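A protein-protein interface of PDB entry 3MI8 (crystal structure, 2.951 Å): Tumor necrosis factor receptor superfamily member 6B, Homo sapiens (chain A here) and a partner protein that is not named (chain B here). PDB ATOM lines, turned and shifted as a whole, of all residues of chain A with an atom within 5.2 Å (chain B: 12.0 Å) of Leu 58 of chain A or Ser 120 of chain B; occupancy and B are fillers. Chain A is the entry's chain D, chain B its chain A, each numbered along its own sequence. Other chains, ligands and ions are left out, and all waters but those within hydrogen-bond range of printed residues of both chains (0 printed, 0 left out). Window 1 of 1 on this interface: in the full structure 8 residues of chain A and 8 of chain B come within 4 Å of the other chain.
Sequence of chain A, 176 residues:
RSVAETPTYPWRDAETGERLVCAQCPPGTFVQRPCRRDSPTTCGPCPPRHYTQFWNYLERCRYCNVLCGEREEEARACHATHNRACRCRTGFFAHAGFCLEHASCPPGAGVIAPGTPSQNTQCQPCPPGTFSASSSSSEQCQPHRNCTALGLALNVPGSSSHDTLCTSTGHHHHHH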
ATOM      1  N   PHE A  30      16.704  14.119  37.285  1.00  0.00           N
ATOM      2  CA  PHE A  30      16.673  15.000  36.124  1.00  0.00           C
ATOM      3  C   PHE A  30      17.478  16.277  36.396  1.00  0.00           C
ATOM      4  O   PHE A  30      17.661  16.661  37.552  1.00  0.00           O
ATOM      5  CB  PHE A  30      15.220  15.351  35.766  1.00  0.00           C
ATOM      6  CG  PHE A  30      14.603  16.401  36.658  1.00  0.00           C
ATOM      7  CD1 PHE A  30      14.497  17.725  36.228  1.00  0.00           C
ATOM      8  CD2 PHE A  30      14.129  16.072  37.922  1.00  0.00           C
ATOM      9  CE1 PHE A  30      13.936  18.707  37.051  1.00  0.00           C
ATOM     10  CE2 PHE A  30      13.563  17.041  38.749  1.00  0.00           C
ATOM     11  CZ  PHE A  30      13.467  18.363  38.312  1.00  0.00           C
ATOM     12  N   VAL A  31      17.928  16.941  35.332  1.00  0.00           N
ATOM     13  CA  VAL A  31      18.652  18.210  35.447  1.00  0.00           C
ATOM     14  C   VAL A  31      17.749  19.328  35.969  1.00  0.00           C
ATOM     15  O   VAL A  31      16.936  19.897  35.232  1.00  0.00           O
ATOM     16  CB  VAL A  31      19.313  18.626  34.107  1.00  0.00           C
ATOM     17  CG1 VAL A  31      20.045  19.963  34.241  1.00  0.00           C
ATOM     18  CG2 VAL A  31      20.279  17.555  33.642  1.00  0.00           C
ATOM     19  N   THR A  52      12.670   8.637  35.085  1.00  0.00           N
ATOM     20  CA  THR A  52      13.746   8.629  34.094  1.00  0.00           C
ATOM     21  C   THR A  52      14.424   7.282  34.250  1.00  0.00           C
ATOM     22  O   THR A  52      14.867   6.936  35.344  1.00  0.00           O
ATOM     23  CB  THR A  52      14.786   9.741  34.319  1.00  0.00           C
ATOM     24  OG1 THR A  52      15.181   9.761  35.697  1.00  0.00           O
ATOM     25  CG2 THR A  52      14.232  11.109  33.919  1.00  0.00           C
ATOM     26  N   TRP A  55      20.446   7.347  32.084  1.00  0.00           N
ATOM     27  CA  TRP A  55      21.274   8.533  32.258  1.00  0.00           C
ATOM     28  C   TRP A  55      20.842   9.564  31.222  1.00  0.00           C
ATOM     29  O   TRP A  55      20.845   9.295  30.019  1.00  0.00           O
ATOM     30  CB  TRP A  55      22.756   8.192  32.094  1.00  0.00           C
ATOM     31  CG  TRP A  55      23.370   7.533  33.290  1.00  0.00           C
ATOM     32  CD1 TRP A  55      23.427   6.191  33.552  1.00  0.00           C
ATOM     33  CD2 TRP A  55      24.028   8.184  34.383  1.00  0.00           C
ATOM     34  NE1 TRP A  55      24.076   5.969  34.743  1.00  0.00           N
ATOM     35  CE2 TRP A  55      24.457   7.175  35.274  1.00  0.00           C
ATOM     36  CE3 TRP A  55      24.298   9.525  34.698  1.00  0.00           C
ATOM     37  CZ2 TRP A  55      25.142   7.463  36.461  1.00  0.00           C
ATOM     38  CZ3 TRP A  55      24.978   9.813  35.877  1.00  0.00           C
ATOM     39  CH2 TRP A  55      25.391   8.785  36.743  1.00  0.00           C
ATOM     40  N   ASN A  56      20.451  10.734  31.703  1.00  0.00           N
ATOM     41  CA  ASN A  56      19.759  11.701  30.871  1.00  0.00           C
ATOM     42  C   ASN A  56      20.174  13.128  31.176  1.00  0.00           C
ATOM     43  O   ASN A  56      20.821  13.389  32.186  1.00  0.00           O
ATOM     44  CB  ASN A  56      18.246  11.568  31.093  1.00  0.00           C
ATOM     45  CG  ASN A  56      17.825  11.990  32.494  1.00  0.00           C
ATOM     46  OD1 ASN A  56      17.432  13.137  32.717  1.00  0.00           O
ATOM     47  ND2 ASN A  56      17.928  11.071  33.447  1.00  0.00           N
ATOM     48  N   TYR A  57      19.779  14.053  30.311  1.00  0.00           N
ATOM     49  CA  TYR A  57      19.814  15.468  30.670  1.00  0.00           C
ATOM     50  C   TYR A  57      18.524  16.196  30.319  1.00  0.00           C
ATOM     51  O   TYR A  57      18.532  17.279  29.725  1.00  0.00           O
ATOM     52  CB  TYR A  57      21.062  16.191  30.156  1.00  0.00           C
ATOM     53  CG  TYR A  57      21.419  16.011  28.696  1.00  0.00           C
ATOM     54  CD1 TYR A  57      21.206  17.042  27.774  1.00  0.00           C
ATOM     55  CD2 TYR A  57      22.017  14.830  28.240  1.00  0.00           C
ATOM     56  CE1 TYR A  57      21.559  16.891  26.434  1.00  0.00           C
ATOM     57  CE2 TYR A  57      22.368  14.663  26.907  1.00  0.00           C
ATOM     58  CZ  TYR A  57      22.142  15.697  26.013  1.00  0.00           C
ATOM     59  OH  TYR A  57      22.496  15.525  24.696  1.00  0.00           O
ATOM     60  N   LEU A  58      17.413  15.580  30.709  1.00  0.00           N
ATOM     61  CA  LEU A  58      16.111  16.209  30.609  1.00  0.00           C
ATOM     62  C   LEU A  58      15.971  17.236  31.713  1.00  0.00           C
ATOM     63  O   LEU A  58      16.510  17.065  32.801  1.00  0.00           O
ATOM     64  CB  LEU A  58      15.006  15.167  30.735  1.00  0.00           C
ATOM     65  CG  LEU A  58      14.978  14.021  29.725  1.00  0.00           C
ATOM     66  CD1 LEU A  58      13.973  12.995  30.182  1.00  0.00           C
ATOM     67  CD2 LEU A  58      14.644  14.519  28.322  1.00  0.00           C
ATOM     68  N   GLU A  59      15.242  18.304  31.424  1.00  0.00           N
ATOM     69  CA  GLU A  59      14.974  19.344  32.401  1.00  0.00           C
ATOM     70  C   GLU A  59      13.619  19.092  33.064  1.00  0.00           C
ATOM     71  O   GLU A  59      13.122  19.913  33.843  1.00  0.00           O
ATOM     72  CB  GLU A  59      15.022  20.714  31.723  1.00  0.00           C
ATOM     73  CG  GLU A  59      16.393  21.045  31.129  1.00  0.00           C
ATOM     74  CD  GLU A  59      16.384  22.270  30.227  1.00  0.00           C
ATOM     75  OE1 GLU A  59      16.890  22.172  29.086  1.00  0.00           O
ATOM     76  OE2 GLU A  59      15.874  23.330  30.654  1.00  0.00           O
ATOM     77  N   ARG A  60      13.050  17.928  32.760  1.00  0.00           N
ATOM     78  CA  ARG A  60      11.720  17.531  33.191  1.00  0.00           C
ATOM     79  C   ARG A  60      11.629  16.012  33.053  1.00  0.00           C
ATOM     80  O   ARG A  60      11.967  15.463  32.003  1.00  0.00           O
ATOM     81  CB  ARG A  60      10.673  18.213  32.304  1.00  0.00           C
ATOM     82  CG  ARG A  60       9.246  18.085  32.780  1.00  0.00           C
ATOM     83  CD  ARG A  60       8.281  18.752  31.813  1.00  0.00           C
ATOM     84  NE  ARG A  60       6.912  18.283  32.025  1.00  0.00           N
ATOM     85  CZ  ARG A  60       5.817  18.882  31.562  1.00  0.00           C
ATOM     86  NH1 ARG A  60       5.908  19.998  30.850  1.00  0.00           N
ATOM     87  NH2 ARG A  60       4.622  18.364  31.822  1.00  0.00           N
ATOM     88  N   CYS A  61      11.192  15.333  34.112  1.00  0.00           N
ATOM     89  CA  CYS A  61      11.053  13.878  34.073  1.00  0.00           C
ATOM     90  C   CYS A  61       9.920  13.455  33.129  1.00  0.00           C
ATOM     91  O   CYS A  61       9.006  14.232  32.854  1.00  0.00           O
ATOM     92  CB  CYS A  61      10.802  13.316  35.475  1.00  0.00           C
ATOM     93  SG  CYS A  61      12.190  13.380  36.646  1.00  0.00           S
ATOM     94  N   ARG A  62       9.994  12.226  32.630  1.00  0.00           N
ATOM     95  CA  ARG A  62       8.937  11.671  31.791  1.00  0.00           C
ATOM     96  C   ARG A  62       7.739  11.228  32.616  1.00  0.00           C
ATOM     97  O   ARG A  62       7.892  10.624  33.669  1.00  0.00           O
ATOM     98  CB  ARG A  62       9.463  10.495  30.987  1.00  0.00           C
ATOM     99  CG  ARG A  62      10.407  10.915  29.910  1.00  0.00           C
ATOM    100  CD  ARG A  62      11.308   9.775  29.511  1.00  0.00           C
ATOM    101  NE  ARG A  62      10.770   8.933  28.442  1.00  0.00           N
ATOM    102  CZ  ARG A  62      10.795   9.242  27.143  1.00  0.00           C
ATOM    103  NH1 ARG A  62      10.290   8.391  26.256  1.00  0.00           N
ATOM    104  NH2 ARG A  62      11.313  10.395  26.723  1.00  0.00           N
ATOM    105  N   LEU B  73      14.318  18.330  11.455  1.00  0.00           N
ATOM    106  CA  LEU B  73      15.061  18.984  12.531  1.00  0.00           C
ATOM    107  C   LEU B  73      14.366  20.276  12.944  1.00  0.00           C
ATOM    108  O   LEU B  73      14.150  21.166  12.118  1.00  0.00           O
ATOM    109  CB  LEU B  73      16.498  19.287  12.083  1.00  0.00           C
ATOM    110  CG  LEU B  73      17.717  19.228  13.026  1.00  0.00           C
ATOM    111  CD1 LEU B  73      18.790  20.186  12.520  1.00  0.00           C
ATOM    112  CD2 LEU B  73      17.430  19.510  14.509  1.00  0.00           C
ATOM    113  N   SER B  77      12.530  26.671  19.234  1.00  0.00           N
ATOM    114  CA  SER B  77      11.606  26.151  20.237  1.00  0.00           C
ATOM    115  C   SER B  77      10.283  26.890  20.184  1.00  0.00           C
ATOM    116  O   SER B  77      10.260  28.104  19.998  1.00  0.00           O
ATOM    117  CB  SER B  77      12.219  26.242  21.628  1.00  0.00           C
ATOM    118  OG  SER B  77      13.408  25.472  21.677  1.00  0.00           O
ATOM    119  N   LYS B 116       8.940  11.952  18.494  1.00  0.00           N
ATOM    120  CA  LYS B 116       9.944  12.962  18.818  1.00  0.00           C
ATOM    121  C   LYS B 116      11.203  12.294  19.389  1.00  0.00           C
ATOM    122  O   LYS B 116      11.119  11.464  20.295  1.00  0.00           O
ATOM    123  CB  LYS B 116       9.386  13.979  19.813  1.00  0.00           C
ATOM    124  CG  LYS B 116      10.321  15.144  20.093  1.00  0.00           C
ATOM    125  CD  LYS B 116       9.769  16.076  21.156  1.00  0.00           C
ATOM    126  CE  LYS B 116       9.912  15.497  22.554  1.00  0.00           C
ATOM    127  NZ  LYS B 116       8.872  16.045  23.473  1.00  0.00           N
ATOM    128  N   VAL B 117      12.360  12.656  18.842  1.00  0.00           N
ATOM    129  CA  VAL B 117      13.649  12.153  19.311  1.00  0.00           C
ATOM    130  C   VAL B 117      14.457  13.335  19.822  1.00  0.00           C
ATOM    131  O   VAL B 117      14.552  14.357  19.148  1.00  0.00           O
ATOM    132  CB  VAL B 117      14.432  11.442  18.179  1.00  0.00           C
ATOM    133  CG1 VAL B 117      15.744  10.879  18.697  1.00  0.00           C
ATOM    134  CG2 VAL B 117      13.589  10.336  17.551  1.00  0.00           C
ATOM    135  N   THR B 118      15.002  13.203  21.031  1.00  0.00           N
ATOM    136  CA  THR B 118      15.919  14.197  21.598  1.00  0.00           C
ATOM    137  C   THR B 118      17.243  13.528  21.954  1.00  0.00           C
ATOM    138  O   THR B 118      17.315  12.305  22.109  1.00  0.00           O
ATOM    139  CB  THR B 118      15.351  14.908  22.861  1.00  0.00           C
ATOM    140  OG1 THR B 118      15.454  14.044  24.001  1.00  0.00           O
ATOM    141  CG2 THR B 118      13.895  15.330  22.666  1.00  0.00           C
ATOM    142  N   ASP B 119      18.293  14.330  22.081  1.00  0.00           N
ATOM    143  CA  ASP B 119      19.586  13.804  22.497  1.00  0.00           C
ATOM    144  C   ASP B 119      19.623  13.629  24.013  1.00  0.00           C
ATOM    145  O   ASP B 119      20.353  12.781  24.533  1.00  0.00           O
ATOM    146  CB  ASP B 119      20.719  14.708  22.007  1.00  0.00           C
ATOM    147  CG  ASP B 119      20.941  14.610  20.503  1.00  0.00           C
ATOM    148  OD1 ASP B 119      20.873  13.485  19.955  1.00  0.00           O
ATOM    149  OD2 ASP B 119      21.186  15.661  19.871  1.00  0.00           O
ATOM    150  N   SER B 120      18.796  14.410  24.705  1.00  0.00           N
ATOM    151  CA  SER B 120      18.740  14.425  26.164  1.00  0.00           C
ATOM    152  C   SER B 120      18.183  13.156  26.817  1.00  0.00           C
ATOM    153  O   SER B 120      18.299  12.995  28.033  1.00  0.00           O
ATOM    154  CB  SER B 120      17.969  15.656  26.645  1.00  0.00           C
ATOM    155  OG  SER B 120      16.742  15.777  25.953  1.00  0.00           O
ATOM    156  N   TYR B 121      17.594  12.261  26.022  1.00  0.00           N
ATOM    157  CA  TYR B 121      17.091  10.975  26.525  1.00  0.00           C
ATOM    158  C   TYR B 121      17.164   9.913  25.418  1.00  0.00           C
ATOM    159  O   TYR B 121      16.834  10.203  24.274  1.00  0.00           O
ATOM    160  CB  TYR B 121      15.657  11.130  27.062  1.00  0.00           C
ATOM    161  CG  TYR B 121      15.163   9.979  27.914  1.00  0.00           C
ATOM    162  CD1 TYR B 121      15.418   9.936  29.284  1.00  0.00           C
ATOM    163  CD2 TYR B 121      14.440   8.928  27.349  1.00  0.00           C
ATOM    164  CE1 TYR B 121      14.963   8.875  30.072  1.00  0.00           C
ATOM    165  CE2 TYR B 121      13.992   7.864  28.122  1.00  0.00           C
ATOM    166  CZ  TYR B 121      14.254   7.843  29.481  1.00  0.00           C
ATOM    167  OH  TYR B 121      13.792   6.790  30.238  1.00  0.00           O
ATOM    168  N   PRO B 122      17.609   8.687  25.753  1.00  0.00           N
ATOM    169  CA  PRO B 122      17.824   7.620  24.767  1.00  0.00           C
ATOM    170  C   PRO B 122      16.567   7.064  24.110  1.00  0.00           C
ATOM    171  O   PRO B 122      16.661   6.429  23.058  1.00  0.00           O
ATOM    172  CB  PRO B 122      18.470   6.503  25.593  1.00  0.00           C
ATOM    173  CG  PRO B 122      19.016   7.168  26.772  1.00  0.00           C
ATOM    174  CD  PRO B 122      18.088   8.280  27.084  1.00  0.00           C
ATOM    175  N   GLU B 123      15.412   7.261  24.736  1.00  0.00           N
ATOM    176  CA  GLU B 123      14.157   6.732  24.203  1.00  0.00           C
ATOM    177  C   GLU B 123      13.309   7.850  23.614  1.00  0.00           C
ATOM    178  O   GLU B 123      13.235   8.952  24.176  1.00  0.00           O
ATOM    179  CB  GLU B 123      13.359   5.961  25.264  1.00  0.00           C
ATOM    180  CG  GLU B 123      14.120   4.839  25.951  1.00  0.00           C
ATOM    181  CD  GLU B 123      13.932   3.473  25.307  1.00  0.00           C
ATOM    182  OE1 GLU B 123      13.570   2.523  26.036  1.00  0.00           O
ATOM    183  OE2 GLU B 123      14.152   3.341  24.083  1.00  0.00           O
ATOM    184  N   PRO B 124      12.664   7.571  22.474  1.00  0.00           N
ATOM    185  CA  PRO B 124      11.814   8.570  21.852  1.00  0.00           C
ATOM    186  C   PRO B 124      10.486   8.779  22.590  1.00  0.00           C
ATOM    187  O   PRO B 124      10.132   7.996  23.475  1.00  0.00           O
ATOM    188  CB  PRO B 124      11.572   7.985  20.462  1.00  0.00           C
ATOM    189  CG  PRO B 124      11.691   6.526  20.632  1.00  0.00           C
ATOM    190  CD  PRO B 124      12.740   6.334  21.673  1.00  0.00           C
ATOM    191  N   THR B 125       9.780   9.846  22.228  1.00  0.00           N
ATOM    192  CA  THR B 125       8.428  10.103  22.710  1.00  0.00           C
ATOM    193  C   THR B 125       7.444   9.892  21.560  1.00  0.00           C
ATOM    194  O   THR B 125       7.656  10.413  20.465  1.00  0.00           O
ATOM    195  CB  THR B 125       8.297  11.545  23.215  1.00  0.00           C
ATOM    196  OG1 THR B 125       9.341  11.818  24.153  1.00  0.00           O
ATOM    197  CG2 THR B 125       6.933  11.781  23.869  1.00  0.00           C
ATOM    198  N   GLN B 126       6.388   9.116  21.798  1.00  0.00           N
ATOM    199  CA  GLN B 126       5.316   8.979  20.815  1.00  0.00           C
ATOM    200  C   GLN B 126       4.335  10.126  20.999  1.00  0.00           C
ATOM    201  O   GLN B 126       3.628  10.194  22.005  1.00  0.00           O
ATOM    202  CB  GLN B 126       4.578   7.650  20.955  1.00  0.00           C
ATOM    203  CG  GLN B 126       5.457   6.428  21.141  1.00  0.00           C
ATOM    204  CD  GLN B 126       4.703   5.132  20.884  1.00  0.00           C
ATOM    205  OE1 GLN B 126       5.189   4.249  20.178  1.00  0.00           O
ATOM    206  NE2 GLN B 126       3.505   5.019  21.449  1.00  0.00           N
ATOM    207  N   LEU B 127       4.307  11.035  20.033  1.00  0.00           N
ATOM    208  CA  LEU B 127       3.401  12.172  20.068  1.00  0.00           C
ATOM    209  C   LEU B 127       1.973  11.781  19.645  1.00  0.00           C
ATOM    210  O   LEU B 127       1.002  12.114  20.325  1.00  0.00           O
ATOM    211  CB  LEU B 127       3.944  13.287  19.174  1.00  0.00           C
ATOM    212  CG  LEU B 127       5.344  13.845  19.447  1.00  0.00           C
ATOM    213  CD1 LEU B 127       5.698  14.839  18.377  1.00  0.00           C
ATOM    214  CD2 LEU B 127       5.432  14.521  20.792  1.00  0.00           C
ATOM    215  N   SER B 152       4.447  21.325  21.899  1.00  0.00           N
ATOM    216  CA  SER B 152       5.549  22.209  22.277  1.00  0.00           C
ATOM    217  C   SER B 152       6.847  21.455  22.060  1.00  0.00           C
ATOM    218  O   SER B 152       7.105  20.456  22.725  1.00  0.00           O
ATOM    219  CB  SER B 152       5.432  22.632  23.739  1.00  0.00           C
ATOM    220  OG  SER B 152       4.174  23.246  23.982  1.00  0.00           O
ATOM    221  N   LEU B 153       7.643  21.917  21.105  1.00  0.00           N
ATOM    222  CA  LEU B 153       8.906  21.273  20.779  1.00  0.00           C
ATOM    223  C   LEU B 153      10.079  22.209  21.050  1.00  0.00           C
ATOM    224  O   LEU B 153       9.905  23.432  21.179  1.00  0.00           O
ATOM    225  CB  LEU B 153       8.924  20.837  19.318  1.00  0.00           C
ATOM    226  CG  LEU B 153       7.751  20.030  18.780  1.00  0.00           C
ATOM    227  CD1 LEU B 153       7.908  19.896  17.288  1.00  0.00           C
ATOM    228  CD2 LEU B 153       7.683  18.667  19.442  1.00  0.00           C
ATOM    229  N   GLN B 154      11.270  21.620  21.122  1.00  0.00           N
ATOM    230  CA  GLN B 154      12.484  22.353  21.463  1.00  0.00           C
ATOM    231  C   GLN B 154      13.488  22.326  20.323  1.00  0.00           C
ATOM    232  O   GLN B 154      13.595  21.331  19.605  1.00  0.00           O
ATOM    233  CB  GLN B 154      13.122  21.749  22.707  1.00  0.00           C
ATOM    234  CG  GLN B 154      12.336  21.956  23.978  1.00  0.00           C
ATOM    235  CD  GLN B 154      12.970  22.982  24.875  1.00  0.00           C
ATOM    236  OE1 GLN B 154      13.446  22.655  25.962  1.00  0.00           O
ATOM    237  NE2 GLN B 154      13.003  24.231  24.423  1.00  0.00           N
ATOM    238  N   GLU B 155      14.219  23.428  20.165  1.00  0.00           N
ATOM    239  CA  GLU B 155      15.312  23.508  19.200  1.00  0.00           C
ATOM    240  C   GLU B 155      16.205  22.291  19.345  1.00  0.00           C
ATOM    241  O   GLU B 155      16.723  22.021  20.426  1.00  0.00           O
ATOM    242  CB  GLU B 155      16.138  24.777  19.427  1.00  0.00           C
ATOM    243  CG  GLU B 155      17.423  24.846  18.595  1.00  0.00           C
ATOM    244  CD  GLU B 155      18.195  26.145  18.776  1.00  0.00           C
ATOM    245  OE1 GLU B 155      19.196  26.340  18.052  1.00  0.00           O
ATOM    246  OE2 GLU B 155      17.810  26.969  19.636  1.00  0.00           O
ATOM    247  N   GLY B 156      16.346  21.541  18.261  1.00  0.00           N
ATOM    248  CA  GLY B 156      17.210  20.377  18.250  1.00  0.00           C
ATOM    249  C   GLY B 156      16.456  19.070  18.182  1.00  0.00           C
ATOM    250  O   GLY B 156      17.060  18.028  17.923  1.00  0.00           O
ATOM    251  N   ASP B 157      15.141  19.122  18.414  1.00  0.00           N
ATOM    252  CA  ASP B 157      14.304  17.922  18.384  1.00  0.00           C
ATOM    253  C   ASP B 157      14.165  17.401  16.968  1.00  0.00           C
ATOM    254  O   ASP B 157      14.142  18.169  16.004  1.00  0.00           O
ATOM    255  CB  ASP B 157      12.913  18.184  18.969  1.00  0.00           C
ATOM    256  CG  ASP B 157      12.935  18.436  20.470  1.00  0.00           C
ATOM    257  OD1 ASP B 157      14.001  18.261  21.099  1.00  0.00           O
ATOM    258  OD2 ASP B 157      11.880  18.825  21.023  1.00  0.00           O
ATOM    259  N   LYS B 158      14.078  16.085  16.853  1.00  0.00           N
ATOM    260  CA  LYS B 158      13.911  15.442  15.568  1.00  0.00           C
ATOM    261  C   LYS B 158      12.541  14.775  15.519  1.00  0.00           C
ATOM    262  O   LYS B 158      12.181  14.033  16.430  1.00  0.00           O
ATOM    263  CB  LYS B 158      15.036  14.424  15.346  1.00  0.00           C
ATOM    264  CG  LYS B 158      16.360  15.042  14.873  1.00  0.00           C
ATOM    265  CD  LYS B 158      17.566  14.159  15.198  1.00  0.00           C
ATOM    266  CE  LYS B 158      18.006  14.347  16.652  1.00  0.00           C
ATOM    267  NZ  LYS B 158      19.293  13.664  16.976  1.00  0.00           N
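No residue of chain B comes within 4 Å of Phe 30 of chain A.
Asn 56 of chain A touches two residues of chain B.
Leu 58 of chain A touches two residues of chain B.
Glu 59 of chain A touches none of the printed residues of chain B.
Of chain B, only Tyr 121, Glu 123, Pro 124 and Thr 125 come within 4 Å of Arg 62 of chain A.
Leu 73 of chain B touches none of the printed residues of chain A.
Ser 120 of chain B touches just these residues of chain A: Asn 56 (3.4 Å), Tyr 57 (2.9 Å) and Leu 58 (3.4 Å).
Printed residues of chain A within 4 Å of Tyr 121 of chain B: Asn 56, Leu 58 and Arg 62.
Printed residues of chain A within 4 Å of Glu 123 of chain B: Arg 62.
Printed residues of chain A within 4 Å of Thr 125 of chain B: Arg 62.
Glu 155 of chain B touches none of the printed residues of chain A.
The nearest residue of chain A that does not touch Ser 120 of chain B is Trp 55 of chain A (4.9 Å).
The nearest printed residue of chain A that does not touch Glu 123 of chain B is Leu 58 of chain A (7.1 Å).
The backbone NH of Lys 116 of chain B is in hydrogen-bond range of the backbone carbonyl oxygen of Thr 125 of chain B (2.8 Å).
The side-chain hydroxyl of Thr 118 of chain B sits at hydrogen-bond distance from the side-chain hydroxyl of Ser 120 of chain B, at 2.9 Å.
The side-chain hydroxyl (OG1) of Thr 118 of chain B is in hydrogen-bond range of the backbone NH (N) of Tyr 121 of chain B, at 3.4 Å.
OD1 of Asp 119 of chain B is in salt-bridge range of NZ of Lys 158 of chain B, at 3.4 Å.
O of Leu 58 of chain A is in hydrogen-bond range of N of Val 31 of chain A, at 2.9 Å.
The side-chain amide oxygen of Asn 56 of chain A is in hydrogen-bond range of the backbone NH of Leu 58 of chain A, 3.2 Å away.
The side-chain hydroxyl (OH) of Tyr 57 of chain A sits close to the backbone carbonyl oxygen (O) of Asp 119 of chain B (3.5 Å).
The backbone carbonyl oxygen (O) of Ser 120 of chain B lies within hydrogen-bond range of the backbone NH (N) of Tyr 57 of chain A, 2.9 Å away.
NH1 of Arg 62 of chain A sits at hydrogen-bond distance from O of Pro 124 of chain B (2.8 Å).
Among the printed residues, pairs that only touch across the chains: Asn 56 of chain A with Ser 120 of chain B, Leu 58 of chain A with Ser 120 of chain B, Arg 62 of chain A with Tyr 121 of chain B, Leu 58 of chain A with Tyr 121 of chain B, Arg 62 of chain A with Glu 123 of chain B, Arg 62 of chain A with Thr 125 of chain B and Asn 56 of chain A with Tyr 121 of chain B.
Of the 21 printed residues of chain B, 6 touch a printed residue of chain A.
Hydrophobic or aromatic side chains of chain B that line the printed part of chain A: Tyr 121.
Of the 11 printed residues of chain A, 4 touch a printed residue of chain B.
Hydrophobic or aromatic side chains of chain A that line the printed part of chain B: Tyr 57 and Leu 58.
Among the printed residues, 10 pairs touch across the chains.
Among the printed residues, no Asp or Glu carboxylate lies within 4 Å of a Lys or Arg side-chain nitrogen of the other chain.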
